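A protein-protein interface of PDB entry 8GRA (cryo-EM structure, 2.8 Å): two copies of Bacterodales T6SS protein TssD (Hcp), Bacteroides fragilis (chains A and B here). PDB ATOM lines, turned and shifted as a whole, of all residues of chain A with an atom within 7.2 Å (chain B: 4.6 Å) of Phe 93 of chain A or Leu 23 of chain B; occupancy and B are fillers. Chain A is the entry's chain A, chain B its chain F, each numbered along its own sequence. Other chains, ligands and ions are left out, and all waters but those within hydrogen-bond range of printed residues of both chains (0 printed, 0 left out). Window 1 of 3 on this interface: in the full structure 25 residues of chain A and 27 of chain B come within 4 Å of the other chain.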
ATOM      1  N   ILE A  54      13.148  15.754 -14.882  1.00  0.00           N
ATOM      2  CA  ILE A  54      12.719  14.763 -13.902  1.00  0.00           C
ATOM      3  C   ILE A  54      13.272  13.392 -14.264  1.00  0.00           C
ATOM      4  O   ILE A  54      13.670  12.617 -13.388  1.00  0.00           O
ATOM      5  CB  ILE A  54      11.183  14.748 -13.788  1.00  0.00           C
ATOM      6  CG1 ILE A  54      10.658  16.117 -13.359  1.00  0.00           C
ATOM      7  CG2 ILE A  54      10.720  13.687 -12.808  1.00  0.00           C
ATOM      8  CD1 ILE A  54       9.219  16.348 -13.731  1.00  0.00           C
ATOM      9  N   LEU A  55      13.305  13.069 -15.560  1.00  0.00           N
ATOM     10  CA  LEU A  55      13.835  11.783 -16.002  1.00  0.00           C
ATOM     11  C   LEU A  55      15.328  11.656 -15.718  1.00  0.00           C
ATOM     12  O   LEU A  55      15.804  10.572 -15.368  1.00  0.00           O
ATOM     13  CB  LEU A  55      13.557  11.584 -17.490  1.00  0.00           C
ATOM     14  CG  LEU A  55      13.776  10.170 -18.024  1.00  0.00           C
ATOM     15  CD1 LEU A  55      13.161   9.142 -17.106  1.00  0.00           C
ATOM     16  CD2 LEU A  55      13.209  10.045 -19.415  1.00  0.00           C
ATOM     17  N   GLU A  56      16.086  12.741 -15.885  1.00  0.00           N
ATOM     18  CA  GLU A  56      17.507  12.695 -15.559  1.00  0.00           C
ATOM     19  C   GLU A  56      17.738  12.480 -14.072  1.00  0.00           C
ATOM     20  O   GLU A  56      18.740  11.873 -13.683  1.00  0.00           O
ATOM     21  CB  GLU A  56      18.195  13.977 -16.011  1.00  0.00           C
ATOM     22  CG  GLU A  56      18.056  14.259 -17.481  1.00  0.00           C
ATOM     23  CD  GLU A  56      18.980  15.359 -17.933  1.00  0.00           C
ATOM     24  OE1 GLU A  56      20.153  15.344 -17.515  1.00  0.00           O
ATOM     25  OE2 GLU A  56      18.536  16.239 -18.698  1.00  0.00           O
ATOM     26  N   MET A  58      15.802  10.629 -12.163  1.00  0.00           N
ATOM     27  CA  MET A  58      15.564   9.209 -11.937  1.00  0.00           C
ATOM     28  C   MET A  58      16.773   8.377 -12.338  1.00  0.00           C
ATOM     29  O   MET A  58      17.170   7.455 -11.616  1.00  0.00           O
ATOM     30  CB  MET A  58      14.322   8.756 -12.701  1.00  0.00           C
ATOM     31  CG  MET A  58      14.161   7.253 -12.769  1.00  0.00           C
ATOM     32  SD  MET A  58      12.489   6.713 -13.140  1.00  0.00           S
ATOM     33  CE  MET A  58      12.411   5.192 -12.208  1.00  0.00           C
ATOM     34  N   THR A  59      17.381   8.693 -13.481  1.00  0.00           N
ATOM     35  CA  THR A  59      18.525   7.927 -13.958  1.00  0.00           C
ATOM     36  C   THR A  59      19.743   8.073 -13.051  1.00  0.00           C
ATOM     37  O   THR A  59      20.645   7.232 -13.105  1.00  0.00           O
ATOM     38  CB  THR A  59      18.865   8.346 -15.387  1.00  0.00           C
ATOM     39  OG1 THR A  59      17.655   8.492 -16.138  1.00  0.00           O
ATOM     40  CG2 THR A  59      19.713   7.292 -16.060  1.00  0.00           C
ATOM     41  N   ILE A  90      12.845   8.742  -6.871  1.00  0.00           N
ATOM     42  CA  ILE A  90      11.765   8.518  -7.826  1.00  0.00           C
ATOM     43  C   ILE A  90      11.779   7.046  -8.207  1.00  0.00           C
ATOM     44  O   ILE A  90      12.787   6.539  -8.707  1.00  0.00           O
ATOM     45  CB  ILE A  90      11.918   9.409  -9.067  1.00  0.00           C
ATOM     46  CG1 ILE A  90      11.852  10.883  -8.679  1.00  0.00           C
ATOM     47  CG2 ILE A  90      10.855   9.084 -10.093  1.00  0.00           C
ATOM     48  CD1 ILE A  90      12.241  11.811  -9.793  1.00  0.00           C
ATOM     49  N   THR A  91      10.664   6.356  -7.972  1.00  0.00           N
ATOM     50  CA  THR A  91      10.603   4.911  -8.147  1.00  0.00           C
ATOM     51  C   THR A  91       9.602   4.471  -9.206  1.00  0.00           C
ATOM     52  O   THR A  91       9.342   3.272  -9.331  1.00  0.00           O
ATOM     53  CB  THR A  91      10.279   4.232  -6.813  1.00  0.00           C
ATOM     54  OG1 THR A  91       9.140   4.857  -6.216  1.00  0.00           O
ATOM     55  CG2 THR A  91      11.459   4.337  -5.868  1.00  0.00           C
ATOM     56  N   GLU A  92       9.033   5.399  -9.969  1.00  0.00           N
ATOM     57  CA  GLU A  92       8.093   5.051 -11.027  1.00  0.00           C
ATOM     58  C   GLU A  92       7.932   6.257 -11.934  1.00  0.00           C
ATOM     59  O   GLU A  92       7.792   7.377 -11.443  1.00  0.00           O
ATOM     60  CB  GLU A  92       6.746   4.631 -10.445  1.00  0.00           C
ATOM     61  CG  GLU A  92       6.101   3.468 -11.163  1.00  0.00           C
ATOM     62  CD  GLU A  92       4.925   2.898 -10.404  1.00  0.00           C
ATOM     63  OE1 GLU A  92       4.918   2.983  -9.158  1.00  0.00           O
ATOM     64  OE2 GLU A  92       4.005   2.360 -11.053  1.00  0.00           O
ATOM     65  N   PHE A  93       7.972   6.035 -13.244  1.00  0.00           N
ATOM     66  CA  PHE A  93       7.895   7.123 -14.208  1.00  0.00           C
ATOM     67  C   PHE A  93       7.107   6.656 -15.422  1.00  0.00           C
ATOM     68  O   PHE A  93       7.330   5.554 -15.924  1.00  0.00           O
ATOM     69  CB  PHE A  93       9.301   7.586 -14.618  1.00  0.00           C
ATOM     70  CG  PHE A  93       9.318   8.646 -15.680  1.00  0.00           C
ATOM     71  CD1 PHE A  93       9.352   8.313 -17.023  1.00  0.00           C
ATOM     72  CD2 PHE A  93       9.331   9.985 -15.331  1.00  0.00           C
ATOM     73  CE1 PHE A  93       9.373   9.291 -17.991  1.00  0.00           C
ATOM     74  CE2 PHE A  93       9.355  10.963 -16.297  1.00  0.00           C
ATOM     75  CZ  PHE A  93       9.378  10.617 -17.625  1.00  0.00           C
ATOM     76  N   THR A  94       6.183   7.493 -15.886  1.00  0.00           N
ATOM     77  CA  THR A  94       5.403   7.213 -17.086  1.00  0.00           C
ATOM     78  C   THR A  94       5.192   8.512 -17.846  1.00  0.00           C
ATOM     79  O   THR A  94       4.850   9.532 -17.245  1.00  0.00           O
ATOM     80  CB  THR A  94       4.046   6.582 -16.746  1.00  0.00           C
ATOM     81  OG1 THR A  94       4.248   5.319 -16.103  1.00  0.00           O
ATOM     82  CG2 THR A  94       3.227   6.361 -17.998  1.00  0.00           C
ATOM     83  N   GLU A  95       5.402   8.479 -19.159  1.00  0.00           N
ATOM     84  CA  GLU A  95       5.141   9.621 -20.023  1.00  0.00           C
ATOM     85  C   GLU A  95       4.213   9.194 -21.150  1.00  0.00           C
ATOM     86  O   GLU A  95       4.520   8.255 -21.888  1.00  0.00           O
ATOM     87  CB  GLU A  95       6.437  10.195 -20.586  1.00  0.00           C
ATOM     88  CG  GLU A  95       6.240  11.026 -21.825  1.00  0.00           C
ATOM     89  CD  GLU A  95       7.139  12.237 -21.857  1.00  0.00           C
ATOM     90  OE1 GLU A  95       8.345  12.093 -21.575  1.00  0.00           O
ATOM     91  OE2 GLU A  95       6.637  13.335 -22.169  1.00  0.00           O
ATOM     92  N   ASN A  96       3.089   9.893 -21.284  1.00  0.00           N
ATOM     93  CA  ASN A  96       2.016   9.517 -22.194  1.00  0.00           C
ATOM     94  C   ASN A  96       1.703  10.660 -23.149  1.00  0.00           C
ATOM     95  O   ASN A  96       1.679  11.825 -22.748  1.00  0.00           O
ATOM     96  CB  ASN A  96       0.760   9.140 -21.415  1.00  0.00           C
ATOM     97  CG  ASN A  96      -0.315   8.561 -22.297  1.00  0.00           C
ATOM     98  OD1 ASN A  96      -0.029   7.890 -23.286  1.00  0.00           O
ATOM     99  ND2 ASN A  96      -1.568   8.822 -21.947  1.00  0.00           N
ATOM    100  N   THR A 106       1.826  14.531 -20.949  1.00  0.00           N
ATOM    101  CA  THR A 106       1.743  14.543 -19.499  1.00  0.00           C
ATOM    102  C   THR A 106       2.746  13.552 -18.928  1.00  0.00           C
ATOM    103  O   THR A 106       3.177  12.617 -19.601  1.00  0.00           O
ATOM    104  CB  THR A 106       0.326  14.203 -19.016  1.00  0.00           C
ATOM    105  OG1 THR A 106      -0.233  13.182 -19.849  1.00  0.00           O
ATOM    106  CG2 THR A 106      -0.573  15.434 -19.059  1.00  0.00           C
ATOM    107  N   ILE A 107       3.119  13.778 -17.670  1.00  0.00           N
ATOM    108  CA  ILE A 107       4.055  12.930 -16.942  1.00  0.00           C
ATOM    109  C   ILE A 107       3.463  12.632 -15.574  1.00  0.00           C
ATOM    110  O   ILE A 107       2.986  13.543 -14.892  1.00  0.00           O
ATOM    111  CB  ILE A 107       5.436  13.597 -16.792  1.00  0.00           C
ATOM    112  CG1 ILE A 107       6.104  13.770 -18.152  1.00  0.00           C
ATOM    113  CG2 ILE A 107       6.323  12.789 -15.881  1.00  0.00           C
ATOM    114  CD1 ILE A 107       7.441  14.445 -18.083  1.00  0.00           C
ATOM    115  N   THR A 108       3.486  11.363 -15.172  1.00  0.00           N
ATOM    116  CA  THR A 108       3.081  10.963 -13.830  1.00  0.00           C
ATOM    117  C   THR A 108       4.190  10.125 -13.205  1.00  0.00           C
ATOM    118  O   THR A 108       4.774   9.270 -13.875  1.00  0.00           O
ATOM    119  CB  THR A 108       1.746  10.201 -13.858  1.00  0.00           C
ATOM    120  OG1 THR A 108       1.455   9.676 -12.559  1.00  0.00           O
ATOM    121  CG2 THR A 108       1.783   9.071 -14.859  1.00  0.00           C
ATOM    122  N   PHE A 109       4.492  10.381 -11.932  1.00  0.00           N
ATOM    123  CA  PHE A 109       5.589   9.698 -11.259  1.00  0.00           C
ATOM    124  C   PHE A 109       5.320   9.624  -9.760  1.00  0.00           C
ATOM    125  O   PHE A 109       4.433  10.296  -9.233  1.00  0.00           O
ATOM    126  CB  PHE A 109       6.935  10.374 -11.563  1.00  0.00           C
ATOM    127  CG  PHE A 109       7.035  11.801 -11.112  1.00  0.00           C
ATOM    128  CD1 PHE A 109       6.376  12.808 -11.791  1.00  0.00           C
ATOM    129  CD2 PHE A 109       7.833  12.141 -10.041  1.00  0.00           C
ATOM    130  CE1 PHE A 109       6.486  14.116 -11.388  1.00  0.00           C
ATOM    131  CE2 PHE A 109       7.946  13.449  -9.635  1.00  0.00           C
ATOM    132  CZ  PHE A 109       7.271  14.436 -10.310  1.00  0.00           C
ATOM    133  N   VAL A 110       6.096   8.778  -9.077  1.00  0.00           N
ATOM    134  CA  VAL A 110       5.937   8.499  -7.652  1.00  0.00           C
ATOM    135  C   VAL A 110       7.261   8.768  -6.946  1.00  0.00           C
ATOM    136  O   VAL A 110       8.330   8.524  -7.508  1.00  0.00           O
ATOM    137  CB  VAL A 110       5.477   7.044  -7.406  1.00  0.00           C
ATOM    138  CG1 VAL A 110       5.082   6.839  -5.966  1.00  0.00           C
ATOM    139  CG2 VAL A 110       4.322   6.681  -8.314  1.00  0.00           C
ATOM    140  N   TYR B  21       5.675   5.195 -22.657  1.00  0.00           N
ATOM    141  CA  TYR B  21       6.761   4.360 -22.147  1.00  0.00           C
ATOM    142  C   TYR B  21       6.902   4.603 -20.648  1.00  0.00           C
ATOM    143  O   TYR B  21       6.454   5.627 -20.130  1.00  0.00           O
ATOM    144  CB  TYR B  21       8.083   4.634 -22.874  1.00  0.00           C
ATOM    145  CG  TYR B  21       8.610   6.034 -22.711  1.00  0.00           C
ATOM    146  CD1 TYR B  21       8.178   7.058 -23.533  1.00  0.00           C
ATOM    147  CD2 TYR B  21       9.548   6.330 -21.739  1.00  0.00           C
ATOM    148  CE1 TYR B  21       8.658   8.336 -23.385  1.00  0.00           C
ATOM    149  CE2 TYR B  21      10.033   7.603 -21.585  1.00  0.00           C
ATOM    150  CZ  TYR B  21       9.586   8.602 -22.409  1.00  0.00           C
ATOM    151  OH  TYR B  21      10.073   9.874 -22.254  1.00  0.00           O
ATOM    152  N   SER B  22       7.535   3.653 -19.957  1.00  0.00           N
ATOM    153  CA  SER B  22       7.544   3.658 -18.499  1.00  0.00           C
ATOM    154  C   SER B  22       8.856   3.099 -17.960  1.00  0.00           C
ATOM    155  O   SER B  22       9.577   2.377 -18.648  1.00  0.00           O
ATOM    156  CB  SER B  22       6.378   2.842 -17.930  1.00  0.00           C
ATOM    157  OG  SER B  22       5.161   3.145 -18.582  1.00  0.00           O
ATOM    158  N   LEU B  23       9.142   3.441 -16.700  1.00  0.00           N
ATOM    159  CA  LEU B  23      10.286   2.935 -15.949  1.00  0.00           C
ATOM    160  C   LEU B  23       9.852   2.662 -14.514  1.00  0.00           C
ATOM    161  O   LEU B  23       8.892   3.254 -14.021  1.00  0.00           O
ATOM    162  CB  LEU B  23      11.455   3.922 -15.968  1.00  0.00           C
ATOM    163  CG  LEU B  23      12.128   4.191 -17.313  1.00  0.00           C
ATOM    164  CD1 LEU B  23      12.950   5.453 -17.248  1.00  0.00           C
ATOM    165  CD2 LEU B  23      12.997   3.026 -17.702  1.00  0.00           C
ATOM    166  N   LYS B  24      10.568   1.763 -13.836  1.00  0.00           N
ATOM    167  CA  LYS B  24      10.138   1.322 -12.512  1.00  0.00           C
ATOM    168  C   LYS B  24      11.320   0.794 -11.709  1.00  0.00           C
ATOM    169  O   LYS B  24      12.338   0.384 -12.262  1.00  0.00           O
ATOM    170  CB  LYS B  24       9.058   0.243 -12.618  1.00  0.00           C
ATOM    171  CG  LYS B  24       8.121   0.172 -11.434  1.00  0.00           C
ATOM    172  CD  LYS B  24       6.971  -0.776 -11.710  1.00  0.00           C
ATOM    173  CE  LYS B  24       5.974  -0.801 -10.561  1.00  0.00           C
ATOM    174  NZ  LYS B  24       6.639  -0.726  -9.229  1.00  0.00           N
ATOM    175  N   ILE B  37      16.754   0.151 -12.056  1.00  0.00           N
ATOM    176  CA  ILE B  37      15.684   0.523 -12.973  1.00  0.00           C
ATOM    177  C   ILE B  37      15.521  -0.555 -14.035  1.00  0.00           C
ATOM    178  O   ILE B  37      16.496  -0.986 -14.662  1.00  0.00           O
ATOM    179  CB  ILE B  37      15.969   1.890 -13.614  1.00  0.00           C
ATOM    180  CG1 ILE B  37      16.014   2.987 -12.556  1.00  0.00           C
ATOM    181  CG2 ILE B  37      14.913   2.235 -14.634  1.00  0.00           C
ATOM    182  CD1 ILE B  37      16.463   4.316 -13.100  1.00  0.00           C
ATOM    183  N   TYR B  38      14.285  -1.003 -14.237  1.00  0.00           N
ATOM    184  CA  TYR B  38      13.949  -1.919 -15.313  1.00  0.00           C
ATOM    185  C   TYR B  38      12.703  -1.418 -16.027  1.00  0.00           C
ATOM    186  O   TYR B  38      11.840  -0.775 -15.425  1.00  0.00           O
ATOM    187  CB  TYR B  38      13.731  -3.350 -14.804  1.00  0.00           C
ATOM    188  CG  TYR B  38      12.712  -3.474 -13.701  1.00  0.00           C
ATOM    189  CD1 TYR B  38      13.087  -3.372 -12.376  1.00  0.00           C
ATOM    190  CD2 TYR B  38      11.377  -3.703 -13.986  1.00  0.00           C
ATOM    191  CE1 TYR B  38      12.164  -3.482 -11.367  1.00  0.00           C
ATOM    192  CE2 TYR B  38      10.445  -3.812 -12.981  1.00  0.00           C
ATOM    193  CZ  TYR B  38      10.847  -3.701 -11.672  1.00  0.00           C
ATOM    194  OH  TYR B  38       9.925  -3.812 -10.660  1.00  0.00           O
ATOM    195  N   GLY B  39      12.621  -1.710 -17.321  1.00  0.00           N
ATOM    196  CA  GLY B  39      11.511  -1.257 -18.133  1.00  0.00           C
ATOM    197  C   GLY B  39      11.944  -0.777 -19.500  1.00  0.00           C
ATOM    198  O   GLY B  39      12.733  -1.443 -20.173  1.00  0.00           O
ATOM    199  N   GLY B  40      11.455   0.384 -19.919  1.00  0.00           N
ATOM    200  CA  GLY B  40      11.792   0.905 -21.233  1.00  0.00           C
ATOM    201  C   GLY B  40      11.165   0.170 -22.399  1.00  0.00           C
ATOM    202  O   GLY B  40      11.855  -0.136 -23.377  1.00  0.00           O
ATOM    203  N   PHE B 123      18.774   5.707 -21.246  1.00  0.00           N
ATOM    204  CA  PHE B 123      18.633   4.506 -20.432  1.00  0.00           C
ATOM    205  C   PHE B 123      19.284   3.338 -21.152  1.00  0.00           C
ATOM    206  O   PHE B 123      18.858   2.972 -22.250  1.00  0.00           O
ATOM    207  CB  PHE B 123      17.165   4.197 -20.136  1.00  0.00           C
ATOM    208  CG  PHE B 123      16.967   2.958 -19.314  1.00  0.00           C
ATOM    209  CD1 PHE B 123      17.531   2.848 -18.059  1.00  0.00           C
ATOM    210  CD2 PHE B 123      16.225   1.899 -19.801  1.00  0.00           C
ATOM    211  CE1 PHE B 123      17.356   1.707 -17.309  1.00  0.00           C
ATOM    212  CE2 PHE B 123      16.047   0.757 -19.052  1.00  0.00           C
ATOM    213  CZ  PHE B 123      16.612   0.662 -17.807  1.00  0.00           C
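The backbone carbonyl oxygen (O) of Phe 93 of chain A is in hydrogen-bond range of the backbone NH (N) of Leu 23 of chain B. The side-chain hydroxyl (OG1) of Thr 94 of chain A is in hydrogen-bond range of the side-chain hydroxyl (OG) of Ser 22 of chain B (3.4 Å). The side-chain carboxylate (OE1) of Glu 95 of chain A is in hydrogen-bond range of the side-chain hydroxyl (OH) of Tyr 21 of chain B (2.9 Å).
The backbone carbonyl oxygen of Leu 55 of chain A lies within hydrogen-bond range of the side-chain hydroxyl of Thr 59 of chain A (2.9 Å). The backbone NH of Thr 91 of chain A is in hydrogen-bond range of the backbone carbonyl oxygen of Val 110 of chain A, at 3.2 Å. O of Glu 92 of chain A sits at hydrogen-bond distance from N of Val 110 of chain A, at 3.2 Å. N of Thr 94 of chain A lies within hydrogen-bond range of O of Thr 108 of chain A (3.0 Å). N of Gly 40 of chain B lies within hydrogen-bond range of O of Ser 22 of chain B (3.0 Å). The backbone NH of Tyr 38 of chain B is in hydrogen-bond range of the backbone carbonyl oxygen of Lys 24 of chain B, 3.1 Å away.
CD1 of Leu 55 of chain A touches CD1 of Leu 23 of chain B (3.7 Å). Met 58 of chain A touches Ile 37 of chain B (O to CD1, 3.5 Å). Thr 91 of chain A touches Lys 24 of chain B. Glu 92 of chain A touches Leu 23 of chain B. Lys 24 of chain B touches Glu 92 of chain A (CE to OE2, 3.8 Å). Phe 93 of chain A touches Ser 22 of chain B. Thr 94 of chain A touches Tyr 21 of chain B (CA to O, 3.6 Å).
Of the printed residues of chain B, Thr 91 of chain A touches Lys 24. Printed residues of chain B within 4 Å of Phe 93 of chain A: Ser 22 (3.2 Å) and Leu 23 (2.9 Å). Of the printed residues of chain B, Glu 95 of chain A touches Tyr 21. Of chain A, only Leu 55 (3.7 Å), Glu 92 (3.6 Å) and Phe 93 (2.9 Å) come within 4 Å of Leu 23 of chain B. Printed residues of chain A within 4 Å of Ile 37 of chain B: Met 58 (3.5 Å). The nearest residue of chain B that does not touch Phe 93 of chain A is Tyr 21 of chain B (4.03 Å).
Of the 9 printed residues of chain B, 5 touch a printed residue of chain A. Of the 17 printed residues of chain A, 7 touch a printed residue of chain B. Printed residues of chain A that touch a printed residue of chain B: Leu 55, Met 58, Thr 91, Glu 92, Phe 93, Thr 94 and Glu 95. Among the printed residues, 10 pairs touch across the chains.
No position is printed for both chains.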
